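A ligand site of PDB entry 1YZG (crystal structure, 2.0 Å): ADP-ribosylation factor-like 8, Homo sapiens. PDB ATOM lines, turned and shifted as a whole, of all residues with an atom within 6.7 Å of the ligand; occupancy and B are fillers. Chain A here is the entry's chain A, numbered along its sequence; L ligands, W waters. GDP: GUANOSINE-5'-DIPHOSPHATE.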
ATOM      1  N   GLY A  23     -15.073  24.210  -3.571  1.00  0.00           N
ATOM      2  CA  GLY A  23     -14.838  22.807  -3.836  1.00  0.00           C
ATOM      3  C   GLY A  23     -16.065  22.056  -3.407  1.00  0.00           C
ATOM      4  O   GLY A  23     -16.901  22.591  -2.690  1.00  0.00           O
ATOM      5  N   LEU A  24     -16.189  20.808  -3.862  1.00  0.00           N
ATOM      6  CA  LEU A  24     -17.279  19.956  -3.360  1.00  0.00           C
ATOM      7  C   LEU A  24     -17.125  19.713  -1.878  1.00  0.00           C
ATOM      8  O   LEU A  24     -16.008  19.860  -1.313  1.00  0.00           O
ATOM      9  CB  LEU A  24     -17.302  18.612  -4.088  1.00  0.00           C
ATOM     10  CG  LEU A  24     -17.392  18.587  -5.629  1.00  0.00           C
ATOM     11  CD1 LEU A  24     -17.098  17.163  -6.089  1.00  0.00           C
ATOM     12  CD2 LEU A  24     -18.746  19.034  -6.122  1.00  0.00           C
ATOM     13  N   ASP A  25     -18.228  19.327  -1.244  1.00  0.00           N
ATOM     14  CA  ASP A  25     -18.166  18.838   0.119  1.00  0.00           C
ATOM     15  C   ASP A  25     -17.142  17.731   0.221  1.00  0.00           C
ATOM     16  O   ASP A  25     -16.988  16.915  -0.709  1.00  0.00           O
ATOM     17  CB  ASP A  25     -19.561  18.392   0.625  1.00  0.00           C
ATOM     18  CG  ASP A  25     -20.046  17.057   0.024  1.00  0.00           C
ATOM     19  OD1 ASP A  25     -20.403  17.022  -1.186  1.00  0.00           O
ATOM     20  OD2 ASP A  25     -20.113  16.046   0.767  1.00  0.00           O
ATOM     21  N   ASN A  26     -16.443  17.694   1.356  1.00  0.00           N
ATOM     22  CA  ASN A  26     -15.397  16.704   1.609  1.00  0.00           C
ATOM     23  C   ASN A  26     -14.103  16.842   0.803  1.00  0.00           C
ATOM     24  O   ASN A  26     -13.274  15.901   0.782  1.00  0.00           O
ATOM     25  CB  ASN A  26     -15.934  15.273   1.502  1.00  0.00           C
ATOM     26  CG  ASN A  26     -15.806  14.523   2.794  1.00  0.00           C
ATOM     27  OD1 ASN A  26     -15.059  13.536   2.885  1.00  0.00           O
ATOM     28  ND2 ASN A  26     -16.477  15.017   3.842  1.00  0.00           N
ATOM     29  N   ALA A  27     -13.918  17.997   0.147  1.00  0.00           N
ATOM     30  CA  ALA A  27     -12.719  18.204  -0.678  1.00  0.00           C
ATOM     31  C   ALA A  27     -11.498  18.431   0.206  1.00  0.00           C
ATOM     32  O   ALA A  27     -10.398  18.022  -0.130  1.00  0.00           O
ATOM     33  CB  ALA A  27     -12.910  19.377  -1.651  1.00  0.00           C
ATOM     34  N   GLY A  28     -11.718  19.097   1.325  1.00  0.00           N
ATOM     35  CA  GLY A  28     -10.653  19.369   2.293  1.00  0.00           C
ATOM     36  C   GLY A  28     -10.515  20.841   2.557  1.00  0.00           C
ATOM     37  O   GLY A  28      -9.531  21.273   3.148  1.00  0.00           O
ATOM     38  N   LYS A  29     -11.513  21.631   2.160  1.00  0.00           N
ATOM     39  CA  LYS A  29     -11.491  23.085   2.334  1.00  0.00           C
ATOM     40  C   LYS A  29     -11.227  23.549   3.776  1.00  0.00           C
ATOM     41  O   LYS A  29     -10.351  24.414   4.007  1.00  0.00           O
ATOM     42  CB  LYS A  29     -12.777  23.728   1.795  1.00  0.00           C
ATOM     43  CG  LYS A  29     -12.966  23.557   0.295  1.00  0.00           C
ATOM     44  CD  LYS A  29     -14.274  24.186  -0.205  1.00  0.00           C
ATOM     45  CE  LYS A  29     -15.500  23.648   0.582  1.00  0.00           C
ATOM     46  NZ  LYS A  29     -15.786  22.186   0.414  1.00  0.00           N
ATOM     47  N   THR A  30     -11.994  23.001   4.711  1.00  0.00           N
ATOM     48  CA  THR A  30     -11.910  23.393   6.129  1.00  0.00           C
ATOM     49  C   THR A  30     -10.548  22.984   6.699  1.00  0.00           C
ATOM     50  O   THR A  30      -9.940  23.737   7.459  1.00  0.00           O
ATOM     51  CB  THR A  30     -13.015  22.720   6.955  1.00  0.00           C
ATOM     52  OG1 THR A  30     -14.274  23.025   6.373  1.00  0.00           O
ATOM     53  CG2 THR A  30     -12.999  23.202   8.407  1.00  0.00           C
ATOM     54  N   THR A  31     -10.075  21.795   6.313  1.00  0.00           N
ATOM     55  CA  THR A  31      -8.778  21.295   6.796  1.00  0.00           C
ATOM     56  C   THR A  31      -7.653  22.179   6.312  1.00  0.00           C
ATOM     57  O   THR A  31      -6.760  22.527   7.074  1.00  0.00           O
ATOM     58  CB  THR A  31      -8.536  19.828   6.376  1.00  0.00           C
ATOM     59  OG1 THR A  31      -9.728  19.079   6.606  1.00  0.00           O
ATOM     60  CG2 THR A  31      -7.369  19.210   7.190  1.00  0.00           C
ATOM     61  N   ILE A  32      -7.669  22.535   5.020  1.00  0.00           N
ATOM     62  CA  ILE A  32      -6.676  23.433   4.449  1.00  0.00           C
ATOM     63  C   ILE A  32      -6.651  24.763   5.219  1.00  0.00           C
ATOM     64  O   ILE A  32      -5.583  25.212   5.680  1.00  0.00           O
ATOM     65  CB  ILE A  32      -6.892  23.629   2.927  1.00  0.00           C
ATOM     66  CG1 ILE A  32      -6.591  22.318   2.183  1.00  0.00           C
ATOM     67  CG2 ILE A  32      -6.093  24.855   2.376  1.00  0.00           C
ATOM     68  CD1 ILE A  32      -6.823  22.341   0.670  1.00  0.00           C
ATOM     69  N   MET A  64     -15.927  31.075   1.884  1.00  0.00           N
ATOM     70  CA  MET A  64     -15.796  29.620   1.706  1.00  0.00           C
ATOM     71  C   MET A  64     -17.154  29.000   1.483  1.00  0.00           C
ATOM     72  O   MET A  64     -18.098  29.314   2.198  1.00  0.00           O
ATOM     73  CB  MET A  64     -15.125  28.972   2.932  1.00  0.00           C
ATOM     74  CG  MET A  64     -14.980  27.433   2.820  1.00  0.00           C
ATOM     75  SD  MET A  64     -14.011  26.649   4.136  1.00  0.00           S
ATOM     76  CE  MET A  64     -12.374  27.112   3.608  1.00  0.00           C
ATOM     77  N   ASP A  66     -19.250  25.182  -0.376  1.00  0.00           N
ATOM     78  CA  ASP A  66     -19.353  23.969  -1.164  1.00  0.00           C
ATOM     79  C   ASP A  66     -20.020  24.251  -2.507  1.00  0.00           C
ATOM     80  O   ASP A  66     -21.062  24.904  -2.566  1.00  0.00           O
ATOM     81  CB  ASP A  66     -20.165  22.909  -0.435  1.00  0.00           C
ATOM     82  CG  ASP A  66     -19.512  22.381   0.818  1.00  0.00           C
ATOM     83  OD1 ASP A  66     -18.261  22.463   1.024  1.00  0.00           O
ATOM     84  OD2 ASP A  66     -20.268  21.859   1.642  1.00  0.00           O
ATOM     85  N   VAL A  90     -10.428  23.518  -4.353  1.00  0.00           N
ATOM     86  CA  VAL A  90      -9.952  22.323  -3.662  1.00  0.00           C
ATOM     87  C   VAL A  90     -10.574  21.096  -4.304  1.00  0.00           C
ATOM     88  O   VAL A  90     -11.795  20.963  -4.369  1.00  0.00           O
ATOM     89  CB  VAL A  90     -10.289  22.337  -2.139  1.00  0.00           C
ATOM     90  CG1 VAL A  90      -9.617  21.146  -1.432  1.00  0.00           C
ATOM     91  CG2 VAL A  90      -9.864  23.670  -1.488  1.00  0.00           C
ATOM     92  N   ASP A  92     -10.703  16.900  -4.331  1.00  0.00           N
ATOM     93  CA  ASP A  92     -10.381  15.602  -3.731  1.00  0.00           C
ATOM     94  C   ASP A  92      -9.822  14.651  -4.812  1.00  0.00           C
ATOM     95  O   ASP A  92     -10.558  14.222  -5.708  1.00  0.00           O
ATOM     96  CB  ASP A  92     -11.627  15.029  -3.039  1.00  0.00           C
ATOM     97  CG  ASP A  92     -11.382  13.666  -2.400  1.00  0.00           C
ATOM     98  OD1 ASP A  92     -10.331  13.037  -2.650  1.00  0.00           O
ATOM     99  OD2 ASP A  92     -12.278  13.221  -1.656  1.00  0.00           O
ATOM    100  N   ASN A 125      -5.837  17.939  -3.692  1.00  0.00           N
ATOM    101  CA  ASN A 125      -5.756  17.550  -2.301  1.00  0.00           C
ATOM    102  C   ASN A 125      -5.879  16.038  -2.221  1.00  0.00           C
ATOM    103  O   ASN A 125      -6.226  15.396  -3.194  1.00  0.00           O
ATOM    104  CB  ASN A 125      -6.855  18.268  -1.500  1.00  0.00           C
ATOM    105  CG  ASN A 125      -6.701  18.106   0.028  1.00  0.00           C
ATOM    106  OD1 ASN A 125      -5.588  18.171   0.580  1.00  0.00           O
ATOM    107  ND2 ASN A 125      -7.815  17.901   0.712  1.00  0.00           N
ATOM    108  N   LYS A 126      -5.553  15.513  -1.049  1.00  0.00           N
ATOM    109  CA  LYS A 126      -5.540  14.076  -0.743  1.00  0.00           C
ATOM    110  C   LYS A 126      -4.556  13.297  -1.620  1.00  0.00           C
ATOM    111  O   LYS A 126      -4.782  12.145  -1.947  1.00  0.00           O
ATOM    112  CB  LYS A 126      -6.928  13.456  -0.748  1.00  0.00           C
ATOM    113  CG  LYS A 126      -8.051  14.380  -0.198  1.00  0.00           C
ATOM    114  CD  LYS A 126      -9.231  13.569   0.275  1.00  0.00           C
ATOM    115  CE  LYS A 126     -10.259  14.454   0.967  1.00  0.00           C
ATOM    116  NZ  LYS A 126     -11.588  13.747   1.068  1.00  0.00           N
ATOM    117  N   GLN A 127      -3.471  13.964  -1.989  1.00  0.00           N
ATOM    118  CA  GLN A 127      -2.399  13.348  -2.760  1.00  0.00           C
ATOM    119  C   GLN A 127      -1.589  12.299  -1.981  1.00  0.00           C
ATOM    120  O   GLN A 127      -0.711  11.628  -2.542  1.00  0.00           O
ATOM    121  CB  GLN A 127      -1.520  14.435  -3.375  1.00  0.00           C
ATOM    122  CG  GLN A 127      -2.135  15.121  -4.611  1.00  0.00           C
ATOM    123  CD  GLN A 127      -2.141  14.222  -5.800  1.00  0.00           C
ATOM    124  OE1 GLN A 127      -1.164  13.499  -6.030  1.00  0.00           O
ATOM    125  NE2 GLN A 127      -3.239  14.235  -6.573  1.00  0.00           N
ATOM    126  N   ASP A 128      -1.918  12.147  -0.697  1.00  0.00           N
ATOM    127  CA  ASP A 128      -1.400  11.074   0.160  1.00  0.00           C
ATOM    128  C   ASP A 128      -2.086   9.740  -0.109  1.00  0.00           C
ATOM    129  O   ASP A 128      -1.534   8.677   0.193  1.00  0.00           O
ATOM    130  CB  ASP A 128      -1.579  11.434   1.638  1.00  0.00           C
ATOM    131  CG  ASP A 128      -3.044  11.593   2.009  1.00  0.00           C
ATOM    132  OD1 ASP A 128      -3.708  12.500   1.482  1.00  0.00           O
ATOM    133  OD2 ASP A 128      -3.535  10.800   2.820  1.00  0.00           O
ATOM    134  N   MET A 129      -3.298   9.787  -0.652  1.00  0.00           N
ATOM    135  CA  MET A 129      -4.096   8.584  -0.867  1.00  0.00           C
ATOM    136  C   MET A 129      -3.589   7.750  -2.058  1.00  0.00           C
ATOM    137  O   MET A 129      -3.361   8.277  -3.155  1.00  0.00           O
ATOM    138  CB  MET A 129      -5.563   8.933  -1.056  1.00  0.00           C
ATOM    139  CG  MET A 129      -6.150   9.700   0.112  1.00  0.00           C
ATOM    140  SD  MET A 129      -7.935   9.658   0.051  1.00  0.00           S
ATOM    141  CE  MET A 129      -8.220   7.976   0.602  1.00  0.00           C
ATOM    142  N   CYS A 157      -1.382  18.604  -2.868  1.00  0.00           N
ATOM    143  CA  CYS A 157      -1.298  18.760  -1.419  1.00  0.00           C
ATOM    144  C   CYS A 157      -1.909  17.617  -0.596  1.00  0.00           C
ATOM    145  O   CYS A 157      -2.593  16.740  -1.124  1.00  0.00           O
ATOM    146  CB  CYS A 157      -1.846  20.118  -0.973  1.00  0.00           C
ATOM    147  SG  CYS A 157      -3.657  20.319  -1.235  1.00  0.00           S
ATOM    148  N   CYS A 158      -1.598  17.616   0.704  1.00  0.00           N
ATOM    149  CA  CYS A 158      -2.255  16.791   1.691  1.00  0.00           C
ATOM    150  C   CYS A 158      -2.623  17.723   2.822  1.00  0.00           C
ATOM    151  O   CYS A 158      -1.766  18.172   3.586  1.00  0.00           O
ATOM    152  CB  CYS A 158      -1.308  15.729   2.242  1.00  0.00           C
ATOM    153  SG  CYS A 158      -2.080  14.761   3.580  1.00  0.00           S
ATOM    154  N   ALA A 159      -3.919  17.996   2.934  1.00  0.00           N
ATOM    155  CA  ALA A 159      -4.402  18.969   3.886  1.00  0.00           C
ATOM    156  C   ALA A 159      -4.093  18.527   5.318  1.00  0.00           C
ATOM    157  O   ALA A 159      -3.770  19.376   6.134  1.00  0.00           O
ATOM    158  CB  ALA A 159      -5.885  19.211   3.701  1.00  0.00           C
ATOM    159  N   LEU A 160      -4.138  17.214   5.578  1.00  0.00           N
ATOM    160  CA  LEU A 160      -3.878  16.663   6.929  1.00  0.00           C
ATOM    161  C   LEU A 160      -2.477  17.000   7.467  1.00  0.00           C
ATOM    162  O   LEU A 160      -2.311  17.371   8.642  1.00  0.00           O
ATOM    163  CB  LEU A 160      -4.116  15.133   6.972  1.00  0.00           C
ATOM    164  CG  LEU A 160      -5.433  14.496   6.528  1.00  0.00           C
ATOM    165  CD1 LEU A 160      -5.312  12.980   6.599  1.00  0.00           C
ATOM    166  CD2 LEU A 160      -6.607  14.957   7.395  1.00  0.00           C
ATOM    167  N   THR A 161      -1.478  16.901   6.612  1.00  0.00           N
ATOM    168  CA  THR A 161      -0.108  17.222   7.014  1.00  0.00           C
ATOM    169  C   THR A 161       0.302  18.646   6.625  1.00  0.00           C
ATOM    170  O   THR A 161       1.367  19.124   7.052  1.00  0.00           O
ATOM    171  CB  THR A 161       0.890  16.263   6.378  1.00  0.00           C
ATOM    172  OG1 THR A 161       0.658  16.278   4.980  1.00  0.00           O
ATOM    173  CG2 THR A 161       0.707  14.822   6.910  1.00  0.00           C
HETATM  174  PB  GDP L   1     -14.606  20.301   3.331  1.00  0.00           P
HETATM  175  O1B GDP L   1     -14.542  21.458   4.282  1.00  0.00           O
HETATM  176  O2B GDP L   1     -14.186  20.662   1.918  1.00  0.00           O
HETATM  177  O3B GDP L   1     -15.995  19.724   3.218  1.00  0.00           O
HETATM  178  O3A GDP L   1     -13.522  19.152   3.680  1.00  0.00           O
HETATM  179  PA  GDP L   1     -12.895  18.822   5.123  1.00  0.00           P
HETATM  180  O1A GDP L   1     -11.816  19.826   5.460  1.00  0.00           O
HETATM  181  O2A GDP L   1     -13.962  18.800   6.186  1.00  0.00           O
HETATM  182  O5' GDP L   1     -12.308  17.365   4.830  1.00  0.00           O
HETATM  183  C5' GDP L   1     -13.253  16.311   4.625  1.00  0.00           C
HETATM  184  C4' GDP L   1     -12.732  14.967   5.085  1.00  0.00           C
HETATM  185  O4' GDP L   1     -11.587  14.541   4.298  1.00  0.00           O
HETATM  186  C3' GDP L   1     -12.279  15.043   6.535  1.00  0.00           C
HETATM  187  O3' GDP L   1     -12.548  13.806   7.191  1.00  0.00           O
HETATM  188  C2' GDP L   1     -10.777  15.233   6.396  1.00  0.00           C
HETATM  189  O2' GDP L   1     -10.067  14.765   7.543  1.00  0.00           O
HETATM  190  C1' GDP L   1     -10.424  14.473   5.129  1.00  0.00           C
HETATM  191  N9  GDP L   1      -9.233  15.045   4.454  1.00  0.00           N
HETATM  192  C8  GDP L   1      -8.982  16.358   4.216  1.00  0.00           C
HETATM  193  N7  GDP L   1      -7.794  16.496   3.557  1.00  0.00           N
HETATM  194  C5  GDP L   1      -7.282  15.259   3.393  1.00  0.00           C
HETATM  195  C6  GDP L   1      -6.068  14.699   2.775  1.00  0.00           C
HETATM  196  O6  GDP L   1      -5.242  15.469   2.265  1.00  0.00           O
HETATM  197  N1  GDP L   1      -5.891  13.360   2.793  1.00  0.00           N
HETATM  198  C2  GDP L   1      -6.805  12.528   3.335  1.00  0.00           C
HETATM  199  N2  GDP L   1      -6.601  11.182   3.335  1.00  0.00           N
HETATM  200  N3  GDP L   1      -7.943  12.985   3.929  1.00  0.00           N
HETATM  201  C4  GDP L   1      -8.219  14.310   3.973  1.00  0.00           C
HETATM  202  O   HOH W   1     -10.767  11.745   3.054  1.00  0.00           O
HETATM  203  O   HOH W   2     -15.020  13.592   7.737  1.00  0.00           O
HETATM  204  O   HOH W   3     -16.063  23.805   3.962  1.00  0.00           O
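An oxygen (O4') of the ligand lies within hydrogen-bond range of the side-chain amino group of Lys 126 (3.3 Å). The side-chain carboxylate of Asp 128 is in hydrogen-bond range of a nitrogen (N1) of the ligand (2.7 Å). N of Asn 26 is in hydrogen-bond range of O3B of the ligand (2.8 Å). N of Lys 29 is in hydrogen-bond range of O2B of the ligand (2.9 Å). An oxygen (O1B) of the ligand lies within hydrogen-bond range of the backbone NH (N) of Thr 30. An oxygen (O6) of the ligand sits close to the side-chain sulfur (SG) of Cys 158 (3.5 Å). O1A of the ligand lies within hydrogen-bond range of OG1 of Thr 31 (2.5 Å). The backbone NH (N) of Ala 159 sits at hydrogen-bond distance from an oxygen (O6) of the ligand, 2.9 Å away. The side-chain hydroxyl (OG1) of Thr 30 lies within hydrogen-bond range of an oxygen (O1B) of the ligand (2.6 Å). The side-chain amide nitrogen (ND2) of Asn 125 lies within hydrogen-bond range of a nitrogen (N7) of the ligand (3.2 Å). O1A of the ligand is in hydrogen-bond range of N of Thr 31 (2.8 Å). The backbone NH (N) of Ala 27 sits at hydrogen-bond distance from an oxygen (O2B) of the ligand. N of Lys 126 sits close to O6 of the ligand (3.3 Å). The backbone NH (N) of Gly 28 is in hydrogen-bond range of an oxygen (O3A) of the ligand (3.0 Å). An oxygen (O2B) of the ligand is in salt-bridge range of the side-chain amino group (NZ) of Lys 29 (2.7 Å).
The side-chain amino group (NZ) of Lys 126 sits at hydrogen-bond distance from the backbone carbonyl oxygen (O) of Asn 26. The backbone carbonyl oxygen (O) of Gly 23 lies within hydrogen-bond range of the side-chain amino group (NZ) of Lys 29 (3.3 Å). OD2 of Asp 92 is in salt-bridge range of NZ of Lys 126 (2.9 Å). ND2 of Asn 125 lies within hydrogen-bond range of O of Ala 27, 2.7 Å away. The backbone carbonyl oxygen (O) of Leu 24 is in hydrogen-bond range of the side-chain amino group (NZ) of Lys 29. N of Ala 159 lies within hydrogen-bond range of OD1 of Asn 125 (2.9 Å). NZ of Lys 29 lies within salt-bridge range of OD1 of Asp 66. The backbone NH (N) of Leu 160 lies close to the side-chain sulfur (SG) of Cys 158, at 3.8 Å.
Leu 24 touches the ligand. Asp 25 touches the ligand (C to O3B, 3.8 Å). Met 129 touches the ligand. Leu 160 touches the ligand. Within 4 Å of the ligand: Leu 24, Asp 25, Asn 26, Ala 27, Gly 28, Lys 29, Thr 30, Thr 31, Asn 125, Lys 126, Asp 128, Met 129, Cys 158, Ala 159 and Leu 160.
Water W3 lies within hydrogen-bond range of O1B of the ligand, OG1 of Thr 30 and SD of Met 64. Water W1 lies within hydrogen-bond range of NZ of Lys 126 (2.9 Å) and O4' of the ligand (3.2 Å).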
